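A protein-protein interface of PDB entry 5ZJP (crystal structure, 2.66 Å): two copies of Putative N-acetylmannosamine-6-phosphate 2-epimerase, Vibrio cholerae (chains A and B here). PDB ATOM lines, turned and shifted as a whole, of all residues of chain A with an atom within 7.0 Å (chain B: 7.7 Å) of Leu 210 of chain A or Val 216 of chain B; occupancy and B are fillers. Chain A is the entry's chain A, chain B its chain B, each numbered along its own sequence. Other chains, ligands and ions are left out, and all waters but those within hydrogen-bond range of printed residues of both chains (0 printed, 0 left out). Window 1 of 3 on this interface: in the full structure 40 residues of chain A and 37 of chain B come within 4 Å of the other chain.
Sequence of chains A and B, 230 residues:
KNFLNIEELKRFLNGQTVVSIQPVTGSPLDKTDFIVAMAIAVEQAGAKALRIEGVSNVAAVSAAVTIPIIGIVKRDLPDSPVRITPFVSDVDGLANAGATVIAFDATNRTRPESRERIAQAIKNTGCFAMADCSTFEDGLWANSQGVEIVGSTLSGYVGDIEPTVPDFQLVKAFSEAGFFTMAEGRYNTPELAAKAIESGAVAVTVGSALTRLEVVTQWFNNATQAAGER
Among the printed residues, pairs that only touch across the chains: Thr 17 of chain A with Phe 220 of chain B, Met 38 of chain A with Leu 213 of chain B, Val 42 of chain A with Leu 213 of chain B, Val 42 of chain A with Thr 217 of chain B, Asn 188 of chain A with Phe 220 of chain B, Pro 190 of chain A with Trp 219 of chain B, Pro 190 of chain A with Phe 220 of chain B, Val 206 of chain A with Phe 220 of chain B, Leu 210 of chain A with Leu 213 of chain B, Leu 210 of chain A with Val 216 of chain B, Leu 210 of chain A with Thr 217 of chain B, Leu 213 of chain A with Leu 210 of chain B and Val 216 of chain A with Leu 210 of chain B.
Of the 18 printed residues of chain B, 7 touch a printed residue of chain A. Printed residues of chain B that touch a printed residue of chain A: Leu 210, Leu 213, Val 216, Thr 217, Trp 219, Phe 220 and Asn 221. Hydrophobic or aromatic side chains of chain B within 4 Å of the printed part of chain A: Leu 210, Leu 213, Val 216 and Phe 220. Among the printed residues, no Asp or Glu carboxylate lies within 4 Å of a Lys or Arg side-chain nitrogen of the other chain.
Leu 210 of chain A touches Leu 213 of chain B, and with the chains exchanged Leu 213 of chain A touches Leu 210 of chain B. Leu 210 of chain A touches Val 216 of chain B, and with the chains exchanged Val 216 of chain A touches Leu 210 of chain B.
Of chain A, only Leu 210 (3.5 Å) comes within 4 Å of Val 216 of chain B. No residue of chain B comes within 4 Å of Ala 209 of chain A. Of the printed residues of chain A, Leu 210 of chain B touches Leu 213 and Val 216. Of the printed residues of chain A, Asn 221 of chain B touches Thr 17 (2.8 Å). Printed residues of chain B within 4 Å of Leu 213 of chain A: Leu 210. Printed residues of chain B within 4 Å of Val 216 of chain A: Leu 210 (3.6 Å). Of the printed residues of chain A, Thr 217 of chain B touches Val 42 (3.6 Å) and Leu 210 (3.8 Å). The nearest residue of chain A that does not touch Val 216 of chain B is Ala 209 of chain A (4.4 Å). The nearest printed residue of chain B that does not touch Val 42 of chain A is Glu 214 of chain B (5.3 Å).
The side-chain amide oxygen (OD1) of Asn 221 of chain B is in hydrogen-bond range of the backbone NH (N) of Thr 17 of chain A (2.8 Å).
O of Leu 213 of chain B lies within hydrogen-bond range of OG1 of Thr 217 of chain B. O of Val 206 of chain A is in hydrogen-bond range of N of Ser 20 of chain A, at 3.0 Å. The backbone carbonyl oxygen of Val 18 of chain A lies within hydrogen-bond range of the backbone NH of Val 206 of chain A.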
ATOM      1  N   THR A  17       7.839   7.194  31.583  1.00  0.00           N
ATOM      2  CA  THR A  17       8.335   6.293  30.553  1.00  0.00           C
ATOM      3  C   THR A  17       9.851   6.215  30.664  1.00  0.00           C
ATOM      4  O   THR A  17      10.529   7.248  30.693  1.00  0.00           O
ATOM      5  CB  THR A  17       7.930   6.765  29.155  1.00  0.00           C
ATOM      6  OG1 THR A  17       6.505   6.727  29.029  1.00  0.00           O
ATOM      7  CG2 THR A  17       8.549   5.873  28.089  1.00  0.00           C
ATOM      8  N   VAL A  18      10.378   4.998  30.722  1.00  0.00           N
ATOM      9  CA  VAL A  18      11.806   4.767  30.905  1.00  0.00           C
ATOM     10  C   VAL A  18      12.393   4.364  29.561  1.00  0.00           C
ATOM     11  O   VAL A  18      11.983   3.357  28.969  1.00  0.00           O
ATOM     12  CB  VAL A  18      12.069   3.692  31.972  1.00  0.00           C
ATOM     13  CG1 VAL A  18      13.549   3.637  32.313  1.00  0.00           C
ATOM     14  CG2 VAL A  18      11.241   3.969  33.217  1.00  0.00           C
ATOM     15  N   VAL A  19      13.352   5.146  29.078  1.00  0.00           N
ATOM     16  CA  VAL A  19      13.898   4.968  27.738  1.00  0.00           C
ATOM     17  C   VAL A  19      15.048   3.973  27.828  1.00  0.00           C
ATOM     18  O   VAL A  19      16.095   4.267  28.410  1.00  0.00           O
ATOM     19  CB  VAL A  19      14.362   6.303  27.144  1.00  0.00           C
ATOM     20  CG1 VAL A  19      15.040   6.078  25.801  1.00  0.00           C
ATOM     21  CG2 VAL A  19      13.187   7.262  27.008  1.00  0.00           C
ATOM     22  N   SER A  20      14.855   2.792  27.245  1.00  0.00           N
ATOM     23  CA  SER A  20      15.906   1.784  27.156  1.00  0.00           C
ATOM     24  C   SER A  20      16.709   2.049  25.888  1.00  0.00           C
ATOM     25  O   SER A  20      16.219   1.825  24.776  1.00  0.00           O
ATOM     26  CB  SER A  20      15.311   0.380  27.155  1.00  0.00           C
ATOM     27  OG  SER A  20      16.317  -0.598  26.957  1.00  0.00           O
ATOM     28  N   MET A  38      22.094  10.086  22.622  1.00  0.00           N
ATOM     29  CA  MET A  38      20.677   9.808  22.842  1.00  0.00           C
ATOM     30  C   MET A  38      20.295   9.992  24.306  1.00  0.00           C
ATOM     31  O   MET A  38      19.206  10.490  24.612  1.00  0.00           O
ATOM     32  CB  MET A  38      20.320   8.400  22.363  1.00  0.00           C
ATOM     33  CG  MET A  38      20.423   8.209  20.855  1.00  0.00           C
ATOM     34  SD  MET A  38      19.794   6.614  20.283  1.00  0.00           S
ATOM     35  CE  MET A  38      21.152   5.524  20.694  1.00  0.00           C
ATOM     36  N   VAL A  42      17.268  12.531  25.400  1.00  0.00           N
ATOM     37  CA  VAL A  42      16.003  12.154  26.027  1.00  0.00           C
ATOM     38  C   VAL A  42      15.846  12.828  27.383  1.00  0.00           C
ATOM     39  O   VAL A  42      14.723  13.120  27.811  1.00  0.00           O
ATOM     40  CB  VAL A  42      15.885  10.623  26.141  1.00  0.00           C
ATOM     41  CG1 VAL A  42      15.789   9.995  24.765  1.00  0.00           C
ATOM     42  CG2 VAL A  42      17.065  10.054  26.901  1.00  0.00           C
ATOM     43  N   ASN A 188       4.840  -0.623  22.289  1.00  0.00           N
ATOM     44  CA  ASN A 188       5.381  -0.042  21.071  1.00  0.00           C
ATOM     45  C   ASN A 188       4.699   1.258  20.663  1.00  0.00           C
ATOM     46  O   ASN A 188       5.147   1.898  19.706  1.00  0.00           O
ATOM     47  CB  ASN A 188       5.266  -1.050  19.921  1.00  0.00           C
ATOM     48  CG  ASN A 188       6.147  -2.266  20.123  1.00  0.00           C
ATOM     49  OD1 ASN A 188       7.133  -2.218  20.859  1.00  0.00           O
ATOM     50  ND2 ASN A 188       5.788  -3.370  19.478  1.00  0.00           N
ATOM     51  N   PRO A 190       2.504   4.912  22.454  1.00  0.00           N
ATOM     52  CA  PRO A 190       2.160   5.588  23.712  1.00  0.00           C
ATOM     53  C   PRO A 190       0.860   5.089  24.312  1.00  0.00           C
ATOM     54  O   PRO A 190       0.659   5.217  25.526  1.00  0.00           O
ATOM     55  CB  PRO A 190       2.060   7.063  23.306  1.00  0.00           C
ATOM     56  CG  PRO A 190       2.929   7.182  22.105  1.00  0.00           C
ATOM     57  CD  PRO A 190       2.801   5.874  21.375  1.00  0.00           C
ATOM     58  N   THR A 205       8.965   0.735  30.570  1.00  0.00           N
ATOM     59  CA  THR A 205      10.208   0.800  29.817  1.00  0.00           C
ATOM     60  C   THR A 205       9.921   0.554  28.342  1.00  0.00           C
ATOM     61  O   THR A 205       9.210  -0.396  27.993  1.00  0.00           O
ATOM     62  CB  THR A 205      11.217  -0.224  30.341  1.00  0.00           C
ATOM     63  OG1 THR A 205      11.502   0.045  31.719  1.00  0.00           O
ATOM     64  CG2 THR A 205      12.514  -0.156  29.547  1.00  0.00           C
ATOM     65  N   VAL A 206      10.472   1.406  27.481  1.00  0.00           N
ATOM     66  CA  VAL A 206      10.287   1.309  26.038  1.00  0.00           C
ATOM     67  C   VAL A 206      11.656   1.399  25.380  1.00  0.00           C
ATOM     68  O   VAL A 206      12.414   2.339  25.642  1.00  0.00           O
ATOM     69  CB  VAL A 206       9.356   2.415  25.503  1.00  0.00           C
ATOM     70  CG1 VAL A 206       9.222   2.314  23.990  1.00  0.00           C
ATOM     71  CG2 VAL A 206       7.991   2.337  26.173  1.00  0.00           C
ATOM     72  N   GLY A 207      11.967   0.428  24.525  1.00  0.00           N
ATOM     73  CA  GLY A 207      13.269   0.375  23.888  1.00  0.00           C
ATOM     74  C   GLY A 207      13.241   0.412  22.373  1.00  0.00           C
ATOM     75  O   GLY A 207      13.692   1.386  21.762  1.00  0.00           O
ATOM     76  N   SER A 208      12.720  -0.655  21.760  1.00  0.00           N
ATOM     77  CA  SER A 208      12.786  -0.795  20.307  1.00  0.00           C
ATOM     78  C   SER A 208      12.064   0.346  19.602  1.00  0.00           C
ATOM     79  O   SER A 208      12.588   0.931  18.647  1.00  0.00           O
ATOM     80  CB  SER A 208      12.200  -2.143  19.885  1.00  0.00           C
ATOM     81  OG  SER A 208      12.974  -3.217  20.391  1.00  0.00           O
ATOM     82  N   ALA A 209      10.852   0.675  20.058  1.00  0.00           N
ATOM     83  CA  ALA A 209      10.071   1.734  19.429  1.00  0.00           C
ATOM     84  C   ALA A 209      10.764   3.091  19.481  1.00  0.00           C
ATOM     85  O   ALA A 209      10.388   3.992  18.724  1.00  0.00           O
ATOM     86  CB  ALA A 209       8.693   1.830  20.086  1.00  0.00           C
ATOM     87  N   LEU A 210      11.759   3.261  20.350  1.00  0.00           N
ATOM     88  CA  LEU A 210      12.435   4.541  20.527  1.00  0.00           C
ATOM     89  C   LEU A 210      13.870   4.565  20.022  1.00  0.00           C
ATOM     90  O   LEU A 210      14.279   5.552  19.409  1.00  0.00           O
ATOM     91  CB  LEU A 210      12.425   4.941  22.008  1.00  0.00           C
ATOM     92  CG  LEU A 210      11.123   5.516  22.567  1.00  0.00           C
ATOM     93  CD1 LEU A 210      11.197   5.648  24.078  1.00  0.00           C
ATOM     94  CD2 LEU A 210      10.850   6.867  21.937  1.00  0.00           C
ATOM     95  N   THR A 211      14.654   3.504  20.248  1.00  0.00           N
ATOM     96  CA  THR A 211      16.097   3.572  20.035  1.00  0.00           C
ATOM     97  C   THR A 211      16.631   2.442  19.157  1.00  0.00           C
ATOM     98  O   THR A 211      17.831   2.151  19.202  1.00  0.00           O
ATOM     99  CB  THR A 211      16.842   3.579  21.375  1.00  0.00           C
ATOM    100  OG1 THR A 211      16.511   2.397  22.116  1.00  0.00           O
ATOM    101  CG2 THR A 211      16.473   4.810  22.196  1.00  0.00           C
ATOM    102  N   ARG A 212      15.779   1.798  18.360  1.00  0.00           N
ATOM    103  CA  ARG A 212      16.215   0.795  17.385  1.00  0.00           C
ATOM    104  C   ARG A 212      15.684   1.208  16.015  1.00  0.00           C
ATOM    105  O   ARG A 212      14.585   0.814  15.620  1.00  0.00           O
ATOM    106  CB  ARG A 212      15.754  -0.606  17.778  1.00  0.00           C
ATOM    107  CG  ARG A 212      16.579  -1.224  18.893  1.00  0.00           C
ATOM    108  CD  ARG A 212      16.023  -2.569  19.326  1.00  0.00           C
ATOM    109  NE  ARG A 212      16.862  -3.194  20.344  1.00  0.00           N
ATOM    110  CZ  ARG A 212      16.441  -4.126  21.191  1.00  0.00           C
ATOM    111  NH1 ARG A 212      15.186  -4.549  21.144  1.00  0.00           N
ATOM    112  NH2 ARG A 212      17.275  -4.637  22.087  1.00  0.00           N
ATOM    113  N   LEU A 213      16.479   2.005  15.296  1.00  0.00           N
ATOM    114  CA  LEU A 213      16.022   2.567  14.027  1.00  0.00           C
ATOM    115  C   LEU A 213      15.775   1.481  12.984  1.00  0.00           C
ATOM    116  O   LEU A 213      14.789   1.546  12.239  1.00  0.00           O
ATOM    117  CB  LEU A 213      17.039   3.589  13.517  1.00  0.00           C
ATOM    118  CG  LEU A 213      16.668   4.354  12.248  1.00  0.00           C
ATOM    119  CD1 LEU A 213      15.387   5.141  12.457  1.00  0.00           C
ATOM    120  CD2 LEU A 213      17.802   5.280  11.842  1.00  0.00           C
ATOM    121  N   VAL A 216      12.352  -0.260  13.735  1.00  0.00           N
ATOM    122  CA  VAL A 216      11.175   0.552  13.439  1.00  0.00           C
ATOM    123  C   VAL A 216      11.040   0.783  11.936  1.00  0.00           C
ATOM    124  O   VAL A 216       9.925   0.816  11.401  1.00  0.00           O
ATOM    125  CB  VAL A 216      11.228   1.880  14.216  1.00  0.00           C
ATOM    126  CG1 VAL A 216       9.924   2.647  14.048  1.00  0.00           C
ATOM    127  CG2 VAL A 216      11.505   1.621  15.686  1.00  0.00           C
ATOM    128  N   TRP A 219       9.312  -2.001  10.554  1.00  0.00           N
ATOM    129  CA  TRP A 219       7.901  -1.941  10.924  1.00  0.00           C
ATOM    130  C   TRP A 219       7.083  -1.169   9.896  1.00  0.00           C
ATOM    131  O   TRP A 219       5.943  -1.542   9.594  1.00  0.00           O
ATOM    132  CB  TRP A 219       7.750  -1.330  12.317  1.00  0.00           C
ATOM    133  CG  TRP A 219       8.108  -2.277  13.422  1.00  0.00           C
ATOM    134  CD1 TRP A 219       8.355  -3.614  13.303  1.00  0.00           C
ATOM    135  CD2 TRP A 219       8.262  -1.962  14.811  1.00  0.00           C
ATOM    136  NE1 TRP A 219       8.649  -4.152  14.532  1.00  0.00           N
ATOM    137  CE2 TRP A 219       8.600  -3.159  15.474  1.00  0.00           C
ATOM    138  CE3 TRP A 219       8.149  -0.786  15.557  1.00  0.00           C
ATOM    139  CZ2 TRP A 219       8.823  -3.212  16.849  1.00  0.00           C
ATOM    140  CZ3 TRP A 219       8.370  -0.842  16.923  1.00  0.00           C
ATOM    141  CH2 TRP A 219       8.703  -2.046  17.553  1.00  0.00           C
ATOM    142  N   VAL B  24      16.189  17.022  15.350  1.00  0.00           N
ATOM    143  CA  VAL B  24      15.732  18.306  15.857  1.00  0.00           C
ATOM    144  C   VAL B  24      16.899  19.282  15.843  1.00  0.00           C
ATOM    145  O   VAL B  24      18.041  18.915  16.153  1.00  0.00           O
ATOM    146  CB  VAL B  24      15.139  18.149  17.267  1.00  0.00           C
ATOM    147  CG1 VAL B  24      14.585  19.472  17.765  1.00  0.00           C
ATOM    148  CG2 VAL B  24      14.054  17.092  17.265  1.00  0.00           C
ATOM    149  N   ASN B 188       2.579   8.818  11.425  1.00  0.00           N
ATOM    150  CA  ASN B 188       3.411   8.542  12.587  1.00  0.00           C
ATOM    151  C   ASN B 188       3.387   7.086  13.044  1.00  0.00           C
ATOM    152  O   ASN B 188       4.124   6.738  13.973  1.00  0.00           O
ATOM    153  CB  ASN B 188       2.995   9.457  13.740  1.00  0.00           C
ATOM    154  CG  ASN B 188       3.309  10.913  13.459  1.00  0.00           C
ATOM    155  OD1 ASN B 188       4.177  11.226  12.644  1.00  0.00           O
ATOM    156  ND2 ASN B 188       2.598  11.811  14.131  1.00  0.00           N
ATOM    157  N   GLY B 207       9.159  10.979   9.045  1.00  0.00           N
ATOM    158  CA  GLY B 207      10.300  11.607   9.682  1.00  0.00           C
ATOM    159  C   GLY B 207      10.333  11.534  11.196  1.00  0.00           C
ATOM    160  O   GLY B 207      11.208  10.878  11.769  1.00  0.00           O
ATOM    161  N   SER B 208       9.389  12.215  11.853  1.00  0.00           N
ATOM    162  CA  SER B 208       9.434  12.354  13.307  1.00  0.00           C
ATOM    163  C   SER B 208       9.388  11.000  14.004  1.00  0.00           C
ATOM    164  O   SER B 208      10.181  10.732  14.913  1.00  0.00           O
ATOM    165  CB  SER B 208       8.280  13.239  13.782  1.00  0.00           C
ATOM    166  OG  SER B 208       8.412  14.557  13.281  1.00  0.00           O
ATOM    167  N   ALA B 209       8.466  10.129  13.586  1.00  0.00           N
ATOM    168  CA  ALA B 209       8.332   8.819  14.215  1.00  0.00           C
ATOM    169  C   ALA B 209       9.596   7.976  14.098  1.00  0.00           C
ATOM    170  O   ALA B 209       9.741   6.994  14.833  1.00  0.00           O
ATOM    171  CB  ALA B 209       7.147   8.065  13.608  1.00  0.00           C
ATOM    172  N   LEU B 210      10.509   8.330  13.196  1.00  0.00           N
ATOM    173  CA  LEU B 210      11.714   7.547  12.954  1.00  0.00           C
ATOM    174  C   LEU B 210      13.000   8.213  13.418  1.00  0.00           C
ATOM    175  O   LEU B 210      13.857   7.540  13.992  1.00  0.00           O
ATOM    176  CB  LEU B 210      11.833   7.223  11.459  1.00  0.00           C
ATOM    177  CG  LEU B 210      10.929   6.104  10.942  1.00  0.00           C
ATOM    178  CD1 LEU B 210      10.969   6.034   9.424  1.00  0.00           C
ATOM    179  CD2 LEU B 210      11.352   4.780  11.548  1.00  0.00           C
ATOM    180  N   THR B 211      13.168   9.523  13.199  1.00  0.00           N
ATOM    181  CA  THR B 211      14.474  10.151  13.385  1.00  0.00           C
ATOM    182  C   THR B 211      14.423  11.392  14.270  1.00  0.00           C
ATOM    183  O   THR B 211      15.352  12.206  14.232  1.00  0.00           O
ATOM    184  CB  THR B 211      15.095  10.518  12.033  1.00  0.00           C
ATOM    185  OG1 THR B 211      14.227  11.418  11.335  1.00  0.00           O
ATOM    186  CG2 THR B 211      15.317   9.273  11.184  1.00  0.00           C
ATOM    187  N   ARG B 212      13.374  11.559  15.074  1.00  0.00           N
ATOM    188  CA  ARG B 212      13.304  12.643  16.057  1.00  0.00           C
ATOM    189  C   ARG B 212      13.019  12.010  17.415  1.00  0.00           C
ATOM    190  O   ARG B 212      11.862  11.860  17.818  1.00  0.00           O
ATOM    191  CB  ARG B 212      12.266  13.691  15.661  1.00  0.00           C
ATOM    192  CG  ARG B 212      12.763  14.614  14.555  1.00  0.00           C
ATOM    193  CD  ARG B 212      11.701  15.586  14.069  1.00  0.00           C
ATOM    194  NE  ARG B 212      12.243  16.500  13.065  1.00  0.00           N
ATOM    195  CZ  ARG B 212      11.509  17.154  12.170  1.00  0.00           C
ATOM    196  NH1 ARG B 212      10.193  17.002  12.147  1.00  0.00           N
ATOM    197  NH2 ARG B 212      12.094  17.963  11.296  1.00  0.00           N
ATOM    198  N   LEU B 213      14.095  11.649  18.118  1.00  0.00           N
ATOM    199  CA  LEU B 213      13.974  10.916  19.374  1.00  0.00           C
ATOM    200  C   LEU B 213      13.257  11.739  20.437  1.00  0.00           C
ATOM    201  O   LEU B 213      12.434  11.208  21.191  1.00  0.00           O
ATOM    202  CB  LEU B 213      15.361  10.495  19.856  1.00  0.00           C
ATOM    203  CG  LEU B 213      15.479   9.640  21.116  1.00  0.00           C
ATOM    204  CD1 LEU B 213      14.739   8.327  20.952  1.00  0.00           C
ATOM    205  CD2 LEU B 213      16.944   9.390  21.419  1.00  0.00           C
ATOM    206  N   GLU B 214      13.570  13.034  20.521  1.00  0.00           N
ATOM    207  CA  GLU B 214      12.890  13.909  21.473  1.00  0.00           C
ATOM    208  C   GLU B 214      11.384  13.901  21.248  1.00  0.00           C
ATOM    209  O   GLU B 214      10.600  13.799  22.200  1.00  0.00           O
ATOM    210  CB  GLU B 214      13.438  15.331  21.355  1.00  0.00           C
ATOM    211  CG  GLU B 214      14.892  15.489  21.767  1.00  0.00           C
ATOM    212  CD  GLU B 214      15.859  15.137  20.649  1.00  0.00           C
ATOM    213  OE1 GLU B 214      15.447  14.457  19.684  1.00  0.00           O
ATOM    214  OE2 GLU B 214      17.035  15.547  20.731  1.00  0.00           O
ATOM    215  N   VAL B 215      10.963  14.021  19.986  1.00  0.00           N
ATOM    216  CA  VAL B 215       9.539  14.080  19.664  1.00  0.00           C
ATOM    217  C   VAL B 215       8.840  12.793  20.087  1.00  0.00           C
ATOM    218  O   VAL B 215       7.782  12.823  20.730  1.00  0.00           O
ATOM    219  CB  VAL B 215       9.343  14.363  18.164  1.00  0.00           C
ATOM    220  CG1 VAL B 215       7.893  14.145  17.765  1.00  0.00           C
ATOM    221  CG2 VAL B 215       9.789  15.779  17.831  1.00  0.00           C
ATOM    222  N   VAL B 216       9.417  11.643  19.732  1.00  0.00           N
ATOM    223  CA  VAL B 216       8.769  10.372  20.042  1.00  0.00           C
ATOM    224  C   VAL B 216       8.805  10.110  21.542  1.00  0.00           C
ATOM    225  O   VAL B 216       7.856   9.556  22.110  1.00  0.00           O
ATOM    226  CB  VAL B 216       9.421   9.226  19.248  1.00  0.00           C
ATOM    227  CG1 VAL B 216       8.620   7.944  19.416  1.00  0.00           C
ATOM    228  CG2 VAL B 216       9.538   9.595  17.782  1.00  0.00           C
ATOM    229  N   THR B 217       9.903  10.486  22.205  1.00  0.00           N
ATOM    230  CA  THR B 217       9.968  10.381  23.660  1.00  0.00           C
ATOM    231  C   THR B 217       8.818  11.135  24.317  1.00  0.00           C
ATOM    232  O   THR B 217       8.122  10.599  25.186  1.00  0.00           O
ATOM    233  CB  THR B 217      11.313  10.909  24.165  1.00  0.00           C
ATOM    234  OG1 THR B 217      12.357  10.002  23.789  1.00  0.00           O
ATOM    235  CG2 THR B 217      11.298  11.060  25.679  1.00  0.00           C
ATOM    236  N   GLN B 218       8.603  12.388  23.906  1.00  0.00           N
ATOM    237  CA  GLN B 218       7.508  13.175  24.463  1.00  0.00           C
ATOM    238  C   GLN B 218       6.147  12.588  24.103  1.00  0.00           C
ATOM    239  O   GLN B 218       5.178  12.785  24.845  1.00  0.00           O
ATOM    240  CB  GLN B 218       7.623  14.627  24.000  1.00  0.00           C
ATOM    241  CG  GLN B 218       8.862  15.330  24.545  1.00  0.00           C
ATOM    242  CD  GLN B 218       8.997  16.759  24.059  1.00  0.00           C
ATOM    243  OE1 GLN B 218       8.513  17.111  22.985  1.00  0.00           O
ATOM    244  NE2 GLN B 218       9.665  17.590  24.852  1.00  0.00           N
ATOM    245  N   TRP B 219       6.050  11.878  22.975  1.00  0.00           N
ATOM    246  CA  TRP B 219       4.800  11.205  22.629  1.00  0.00           C
ATOM    247  C   TRP B 219       4.412  10.164  23.675  1.00  0.00           C
ATOM    248  O   TRP B 219       3.229  10.019  24.004  1.00  0.00           O
ATOM    249  CB  TRP B 219       4.911  10.553  21.249  1.00  0.00           C
ATOM    250  CG  TRP B 219       4.811  11.510  20.102  1.00  0.00           C
ATOM    251  CD1 TRP B 219       4.465  12.828  20.161  1.00  0.00           C
ATOM    252  CD2 TRP B 219       5.053  11.219  18.720  1.00  0.00           C
ATOM    253  NE1 TRP B 219       4.480  13.377  18.902  1.00  0.00           N
ATOM    254  CE2 TRP B 219       4.838  12.410  17.999  1.00  0.00           C
ATOM    255  CE3 TRP B 219       5.432  10.068  18.024  1.00  0.00           C
ATOM    256  CZ2 TRP B 219       4.988  12.483  16.616  1.00  0.00           C
ATOM    257  CZ3 TRP B 219       5.583  10.142  16.650  1.00  0.00           C
ATOM    258  CH2 TRP B 219       5.362  11.342  15.963  1.00  0.00           C
ATOM    259  N   PHE B 220       5.393   9.432  24.211  1.00  0.00           N
ATOM    260  CA  PHE B 220       5.090   8.387  25.187  1.00  0.00           C
ATOM    261  C   PHE B 220       4.833   8.957  26.577  1.00  0.00           C
ATOM    262  O   PHE B 220       3.833   8.612  27.217  1.00  0.00           O
ATOM    263  CB  PHE B 220       6.221   7.358  25.240  1.00  0.00           C
ATOM    264  CG  PHE B 220       6.278   6.445  24.046  1.00  0.00           C
ATOM    265  CD1 PHE B 220       6.405   6.948  22.762  1.00  0.00           C
ATOM    266  CD2 PHE B 220       6.194   5.073  24.215  1.00  0.00           C
ATOM    267  CE1 PHE B 220       6.452   6.103  21.673  1.00  0.00           C
ATOM    268  CE2 PHE B 220       6.241   4.223  23.131  1.00  0.00           C
ATOM    269  CZ  PHE B 220       6.369   4.736  21.859  1.00  0.00           C
ATOM    270  N   ASN B 221       5.733   9.814  27.068  1.00  0.00           N
ATOM    271  CA  ASN B 221       5.546  10.398  28.394  1.00  0.00           C
ATOM    272  C   ASN B 221       4.243  11.178  28.495  1.00  0.00           C
ATOM    273  O   ASN B 221       3.614  11.191  29.557  1.00  0.00           O
ATOM    274  CB  ASN B 221       6.731  11.295  28.755  1.00  0.00           C
ATOM    275  CG  ASN B 221       7.748  10.591  29.632  1.00  0.00           C
ATOM    276  OD1 ASN B 221       7.421   9.636  30.336  1.00  0.00           O
ATOM    277  ND2 ASN B 221       8.990  11.061  29.595  1.00  0.00           N
ATOM    278  N   ASN B 222       3.822  11.831  27.410  1.00  0.00           N
ATOM    279  CA  ASN B 222       2.545  12.540  27.427  1.00  0.00           C
ATOM    280  C   ASN B 222       1.396  11.598  27.772  1.00  0.00           C
ATOM    281  O   ASN B 222       0.473  11.974  28.505  1.00  0.00           O
ATOM    282  CB  ASN B 222       2.303  13.222  26.080  1.00  0.00           C
ATOM    283  CG  ASN B 222       1.311  14.368  26.171  1.00  0.00           C
ATOM    284  OD1 ASN B 222       0.392  14.348  26.989  1.00  0.00           O
ATOM    285  ND2 ASN B 222       1.494  15.377  25.326  1.00  0.00           N
